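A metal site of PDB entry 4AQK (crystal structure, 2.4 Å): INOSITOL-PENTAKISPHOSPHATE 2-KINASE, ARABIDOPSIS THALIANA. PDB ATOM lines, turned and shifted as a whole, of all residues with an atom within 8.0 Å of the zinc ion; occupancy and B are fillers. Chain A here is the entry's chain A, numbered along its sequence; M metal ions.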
ATOM      1  N   GLU A 321      -1.903   9.201 -28.404  1.00  0.00           N
ATOM      2  CA  GLU A 321      -1.018   8.359 -29.213  1.00  0.00           C
ATOM      3  C   GLU A 321      -0.072   7.526 -28.357  1.00  0.00           C
ATOM      4  O   GLU A 321       0.458   6.504 -28.808  1.00  0.00           O
ATOM      5  CB  GLU A 321      -0.224   9.207 -30.205  1.00  0.00           C
ATOM      6  CG  GLU A 321      -1.065   9.852 -31.290  1.00  0.00           C
ATOM      7  CD  GLU A 321      -0.260  10.218 -32.510  1.00  0.00           C
ATOM      8  OE1 GLU A 321      -0.057   9.334 -33.363  1.00  0.00           O
ATOM      9  OE2 GLU A 321       0.171  11.386 -32.628  1.00  0.00           O
ATOM     10  N   GLY A 322       0.148   7.980 -27.125  1.00  0.00           N
ATOM     11  CA  GLY A 322       0.844   7.186 -26.123  1.00  0.00           C
ATOM     12  C   GLY A 322      -0.160   6.283 -25.442  1.00  0.00           C
ATOM     13  O   GLY A 322      -0.170   5.076 -25.668  1.00  0.00           O
ATOM     14  N   ILE A 324      -3.047   5.127 -25.671  1.00  0.00           N
ATOM     15  CA  ILE A 324      -3.818   4.094 -26.370  1.00  0.00           C
ATOM     16  C   ILE A 324      -3.190   2.693 -26.257  1.00  0.00           C
ATOM     17  O   ILE A 324      -3.898   1.699 -26.255  1.00  0.00           O
ATOM     18  CB  ILE A 324      -4.050   4.453 -27.871  1.00  0.00           C
ATOM     19  CG1 ILE A 324      -5.022   3.480 -28.546  1.00  0.00           C
ATOM     20  CG2 ILE A 324      -2.732   4.497 -28.640  1.00  0.00           C
ATOM     21  CD1 ILE A 324      -6.491   3.657 -28.154  1.00  0.00           C
ATOM     22  N   HIS A 325      -1.859   2.644 -26.152  1.00  0.00           N
ATOM     23  CA  HIS A 325      -1.138   1.380 -26.052  1.00  0.00           C
ATOM     24  C   HIS A 325      -1.368   0.730 -24.690  1.00  0.00           C
ATOM     25  O   HIS A 325      -1.679  -0.445 -24.603  1.00  0.00           O
ATOM     26  CB  HIS A 325       0.356   1.589 -26.317  1.00  0.00           C
ATOM     27  CG  HIS A 325       0.645   2.105 -27.691  1.00  0.00           C
ATOM     28  ND1 HIS A 325       0.863   1.263 -28.765  1.00  0.00           N
ATOM     29  CD2 HIS A 325       0.700   3.362 -28.177  1.00  0.00           C
ATOM     30  CE1 HIS A 325       1.069   1.990 -29.848  1.00  0.00           C
ATOM     31  NE2 HIS A 325       0.969   3.268 -29.518  1.00  0.00           N
ATOM     32  N   CYS A 326      -1.240   1.532 -23.631  1.00  0.00           N
ATOM     33  CA  CYS A 326      -1.519   1.067 -22.275  1.00  0.00           C
ATOM     34  C   CYS A 326      -2.945   0.579 -22.153  1.00  0.00           C
ATOM     35  O   CYS A 326      -3.224  -0.350 -21.403  1.00  0.00           O
ATOM     36  CB  CYS A 326      -1.263   2.184 -21.270  1.00  0.00           C
ATOM     37  SG  CYS A 326       0.315   3.008 -21.535  1.00  0.00           S
ATOM     38  N   TYR A 327      -3.855   1.193 -22.922  1.00  0.00           N
ATOM     39  CA  TYR A 327      -5.261   0.801 -22.917  1.00  0.00           C
ATOM     40  C   TYR A 327      -5.470  -0.670 -23.307  1.00  0.00           C
ATOM     41  O   TYR A 327      -6.254  -1.366 -22.663  1.00  0.00           O
ATOM     42  CB  TYR A 327      -6.106   1.741 -23.798  1.00  0.00           C
ATOM     43  CG  TYR A 327      -7.491   1.213 -24.123  1.00  0.00           C
ATOM     44  CD1 TYR A 327      -8.528   1.263 -23.184  1.00  0.00           C
ATOM     45  CD2 TYR A 327      -7.774   0.668 -25.370  1.00  0.00           C
ATOM     46  CE1 TYR A 327      -9.805   0.786 -23.485  1.00  0.00           C
ATOM     47  CE2 TYR A 327      -9.039   0.178 -25.680  1.00  0.00           C
ATOM     48  CZ  TYR A 327     -10.047   0.249 -24.736  1.00  0.00           C
ATOM     49  OH  TYR A 327     -11.294  -0.229 -25.040  1.00  0.00           O
ATOM     50  N   TYR A 328      -4.772  -1.131 -24.353  1.00  0.00           N
ATOM     51  CA  TYR A 328      -4.901  -2.525 -24.794  1.00  0.00           C
ATOM     52  C   TYR A 328      -4.296  -3.535 -23.815  1.00  0.00           C
ATOM     53  O   TYR A 328      -4.830  -4.632 -23.651  1.00  0.00           O
ATOM     54  CB  TYR A 328      -4.352  -2.726 -26.204  1.00  0.00           C
ATOM     55  CG  TYR A 328      -5.174  -2.028 -27.254  1.00  0.00           C
ATOM     56  CD1 TYR A 328      -6.449  -2.489 -27.598  1.00  0.00           C
ATOM     57  CD2 TYR A 328      -4.686  -0.902 -27.906  1.00  0.00           C
ATOM     58  CE1 TYR A 328      -7.222  -1.838 -28.555  1.00  0.00           C
ATOM     59  CE2 TYR A 328      -5.448  -0.241 -28.864  1.00  0.00           C
ATOM     60  CZ  TYR A 328      -6.708  -0.717 -29.187  1.00  0.00           C
ATOM     61  OH  TYR A 328      -7.451  -0.067 -30.148  1.00  0.00           O
ATOM     62  N   ASP A 329      -3.199  -3.154 -23.163  1.00  0.00           N
ATOM     63  CA  ASP A 329      -2.615  -4.012 -22.126  1.00  0.00           C
ATOM     64  C   ASP A 329      -3.599  -4.181 -20.970  1.00  0.00           C
ATOM     65  O   ASP A 329      -3.739  -5.271 -20.420  1.00  0.00           O
ATOM     66  CB  ASP A 329      -1.301  -3.425 -21.604  1.00  0.00           C
ATOM     67  CG  ASP A 329      -0.280  -3.158 -22.701  1.00  0.00           C
ATOM     68  OD1 ASP A 329      -0.371  -3.793 -23.781  1.00  0.00           O
ATOM     69  OD2 ASP A 329       0.614  -2.327 -22.479  1.00  0.00           O
ATOM     70  N   GLN A 333      -5.477  -7.178 -24.521  1.00  0.00           N
ATOM     71  CA  GLN A 333      -5.724  -7.367 -25.939  1.00  0.00           C
ATOM     72  C   GLN A 333      -4.457  -7.074 -26.724  1.00  0.00           C
ATOM     73  O   GLN A 333      -3.734  -6.127 -26.408  1.00  0.00           O
ATOM     74  CB  GLN A 333      -6.867  -6.464 -26.399  1.00  0.00           C
ATOM     75  CG  GLN A 333      -7.659  -7.017 -27.553  1.00  0.00           C
ATOM     76  CD  GLN A 333      -8.637  -6.008 -28.133  1.00  0.00           C
ATOM     77  OE1 GLN A 333      -9.675  -5.719 -27.532  1.00  0.00           O
ATOM     78  NE2 GLN A 333      -8.309  -5.481 -29.313  1.00  0.00           N
ATOM     79  N   PRO A 334      -4.155  -7.908 -27.740  1.00  0.00           N
ATOM     80  CA  PRO A 334      -3.019  -7.645 -28.612  1.00  0.00           C
ATOM     81  C   PRO A 334      -3.181  -6.292 -29.286  1.00  0.00           C
ATOM     82  O   PRO A 334      -4.140  -6.092 -30.040  1.00  0.00           O
ATOM     83  CB  PRO A 334      -3.104  -8.771 -29.644  1.00  0.00           C
ATOM     84  CG  PRO A 334      -3.832  -9.865 -28.956  1.00  0.00           C
ATOM     85  CD  PRO A 334      -4.819  -9.187 -28.062  1.00  0.00           C
ATOM     86  N   CYS A 335      -2.276  -5.365 -28.989  1.00  0.00           N
ATOM     87  CA  CYS A 335      -2.341  -3.989 -29.477  1.00  0.00           C
ATOM     88  C   CYS A 335      -2.414  -3.926 -30.995  1.00  0.00           C
ATOM     89  O   CYS A 335      -1.461  -4.305 -31.665  1.00  0.00           O
ATOM     90  CB  CYS A 335      -1.142  -3.187 -28.960  1.00  0.00           C
ATOM     91  SG  CYS A 335      -0.983  -1.490 -29.606  1.00  0.00           S
ATOM     92  N   PRO A 336      -3.555  -3.486 -31.546  1.00  0.00           N
ATOM     93  CA  PRO A 336      -3.697  -3.354 -32.990  1.00  0.00           C
ATOM     94  C   PRO A 336      -2.900  -2.193 -33.595  1.00  0.00           C
ATOM     95  O   PRO A 336      -2.740  -2.153 -34.811  1.00  0.00           O
ATOM     96  CB  PRO A 336      -5.197  -3.110 -33.189  1.00  0.00           C
ATOM     97  CG  PRO A 336      -5.642  -2.531 -31.913  1.00  0.00           C
ATOM     98  CD  PRO A 336      -4.833  -3.225 -30.864  1.00  0.00           C
ATOM     99  N   ILE A 337      -2.413  -1.272 -32.772  1.00  0.00           N
ATOM    100  CA  ILE A 337      -1.607  -0.167 -33.281  1.00  0.00           C
ATOM    101  C   ILE A 337      -0.169  -0.636 -33.569  1.00  0.00           C
ATOM    102  O   ILE A 337       0.374  -0.374 -34.648  1.00  0.00           O
ATOM    103  CB  ILE A 337      -1.578   1.065 -32.326  1.00  0.00           C
ATOM    104  CG1 ILE A 337      -2.952   1.353 -31.703  1.00  0.00           C
ATOM    105  CG2 ILE A 337      -0.993   2.291 -33.043  1.00  0.00           C
ATOM    106  CD1 ILE A 337      -4.062   1.732 -32.681  1.00  0.00           C
ATOM    107  N   CYS A 338       0.424  -1.344 -32.611  1.00  0.00           N
ATOM    108  CA  CYS A 338       1.764  -1.917 -32.763  1.00  0.00           C
ATOM    109  C   CYS A 338       1.775  -3.022 -33.809  1.00  0.00           C
ATOM    110  O   CYS A 338       2.661  -3.071 -34.660  1.00  0.00           O
ATOM    111  CB  CYS A 338       2.299  -2.413 -31.413  1.00  0.00           C
ATOM    112  SG  CYS A 338       2.614  -1.078 -30.230  1.00  0.00           S
ATOM    113  N   ARG A 339       0.778  -3.909 -33.726  1.00  0.00           N
ATOM    114  CA  ARG A 339       0.435  -4.804 -34.822  1.00  0.00           C
ATOM    115  C   ARG A 339      -0.151  -3.928 -35.933  1.00  0.00           C
ATOM    116  O   ARG A 339      -0.555  -2.804 -35.667  1.00  0.00           O
ATOM    117  CB  ARG A 339      -0.607  -5.829 -34.390  1.00  0.00           C
ATOM    118  CG  ARG A 339      -0.064  -7.059 -33.682  1.00  0.00           C
ATOM    119  CD  ARG A 339      -1.151  -8.117 -33.576  1.00  0.00           C
ATOM    120  NE  ARG A 339      -0.642  -9.484 -33.629  1.00  0.00           N
ATOM    121  CZ  ARG A 339      -0.312 -10.138 -34.745  1.00  0.00           C
ATOM    122  NH1 ARG A 339      -0.422  -9.546 -35.937  1.00  0.00           N
ATOM    123  NH2 ARG A 339       0.138 -11.382 -34.680  1.00  0.00           N
ATOM    124  N   GLU A 345       8.746   0.140 -34.998  1.00  0.00           N
ATOM    125  CA  GLU A 345       8.104   1.441 -34.799  1.00  0.00           C
ATOM    126  C   GLU A 345       7.020   0.995 -33.810  1.00  0.00           C
ATOM    127  O   GLU A 345       6.168   1.788 -33.401  1.00  0.00           O
ATOM    128  CB  GLU A 345       7.481   2.221 -35.951  1.00  0.00           C
ATOM    129  CG  GLU A 345       8.480   2.886 -36.867  1.00  0.00           C
ATOM    130  CD  GLU A 345       7.821   3.589 -38.040  1.00  0.00           C
ATOM    131  OE1 GLU A 345       6.643   3.274 -38.339  1.00  0.00           O
ATOM    132  OE2 GLU A 345       8.476   4.465 -38.655  1.00  0.00           O
ATOM    133  N   ALA A 346       7.063  -0.282 -33.454  1.00  0.00           N
ATOM    134  CA  ALA A 346       6.259  -0.792 -32.353  1.00  0.00           C
ATOM    135  C   ALA A 346       6.678  -0.050 -31.083  1.00  0.00           C
ATOM    136  O   ALA A 346       7.873   0.070 -30.784  1.00  0.00           O
ATOM    137  CB  ALA A 346       6.449  -2.281 -32.201  1.00  0.00           C
ATOM    138  N   GLU A 347       5.686   0.467 -30.359  1.00  0.00           N
ATOM    139  CA  GLU A 347       5.947   1.270 -29.168  1.00  0.00           C
ATOM    140  C   GLU A 347       6.249   0.350 -27.967  1.00  0.00           C
ATOM    141  O   GLU A 347       5.371   0.024 -27.172  1.00  0.00           O
ATOM    142  CB  GLU A 347       4.763   2.212 -28.911  1.00  0.00           C
ATOM    143  CG  GLU A 347       5.142   3.546 -28.290  1.00  0.00           C
ATOM    144  CD  GLU A 347       5.954   4.453 -29.214  1.00  0.00           C
ATOM    145  OE1 GLU A 347       5.407   4.909 -30.250  1.00  0.00           O
ATOM    146  OE2 GLU A 347       7.141   4.706 -28.899  1.00  0.00           O
ATOM    147  N   LEU A 348       7.511  -0.060 -27.862  1.00  0.00           N
ATOM    148  CA  LEU A 348       7.928  -1.133 -26.952  1.00  0.00           C
ATOM    149  C   LEU A 348       8.044  -0.717 -25.489  1.00  0.00           C
ATOM    150  O   LEU A 348       7.724  -1.499 -24.587  1.00  0.00           O
ATOM    151  CB  LEU A 348       9.263  -1.742 -27.416  1.00  0.00           C
ATOM    152  CG  LEU A 348       9.372  -2.312 -28.840  1.00  0.00           C
ATOM    153  CD1 LEU A 348      10.818  -2.699 -29.175  1.00  0.00           C
ATOM    154  CD2 LEU A 348       8.435  -3.490 -29.051  1.00  0.00           C
ATOM    155  N   LEU A 350       6.253   1.409 -23.844  1.00  0.00           N
ATOM    156  CA  LEU A 350       4.941   1.454 -23.222  1.00  0.00           C
ATOM    157  C   LEU A 350       4.423   0.061 -22.862  1.00  0.00           C
ATOM    158  O   LEU A 350       3.929  -0.147 -21.751  1.00  0.00           O
ATOM    159  CB  LEU A 350       3.938   2.178 -24.125  1.00  0.00           C
ATOM    160  CG  LEU A 350       4.134   3.689 -24.286  1.00  0.00           C
ATOM    161  CD1 LEU A 350       3.168   4.232 -25.318  1.00  0.00           C
ATOM    162  CD2 LEU A 350       4.020   4.456 -22.960  1.00  0.00           C
ATOM    163  N   HIS A 351       4.552  -0.893 -23.774  1.00  0.00           N
ATOM    164  CA  HIS A 351       4.092  -2.261 -23.530  1.00  0.00           C
ATOM    165  C   HIS A 351       4.933  -3.033 -22.504  1.00  0.00           C
ATOM    166  O   HIS A 351       4.478  -4.034 -21.950  1.00  0.00           O
ATOM    167  CB  HIS A 351       3.982  -3.026 -24.844  1.00  0.00           C
ATOM    168  CG  HIS A 351       2.874  -2.529 -25.728  1.00  0.00           C
ATOM    169  ND1 HIS A 351       1.542  -2.700 -25.416  1.00  0.00           N
ATOM    170  CD2 HIS A 351       2.895  -1.860 -26.904  1.00  0.00           C
ATOM    171  CE1 HIS A 351       0.800  -2.164 -26.360  1.00  0.00           C
ATOM    172  NE2 HIS A 351       1.592  -1.651 -27.282  1.00  0.00           N
HETATM  173 ZN    ZN M   1       0.920  -0.831 -28.940  1.00  0.00          ZN
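The side-chain carboxylate (OD1) of Asp 329 lies within hydrogen-bond range of a ring nitrogen (ND1) of His 351.
The backbone carbonyl oxygen (O) of Glu 321 sits close to a ring nitrogen (NE2) of His 325 (3.4 Å).
The backbone NH of Ile 337 lies close to the side-chain sulfur of Cys 335 (3.5 Å).
The side-chain sulfur of Cys 338 sits close to the backbone NH of Glu 347, at 3.4 Å.
Within 4 Å of the zinc ion: His 325, Cys 335, Cys 338 and His 351.
The nearest printed residue that does not touch the zinc ion is Ile 337 (4.6 Å).
The zinc ion is bound by NE2 of His 351 (2.0 Å), ND1 of His 325 (2.1 Å), SG of Cys 335 (2.1 Å) and SG of Cys 338 (2.1 Å).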
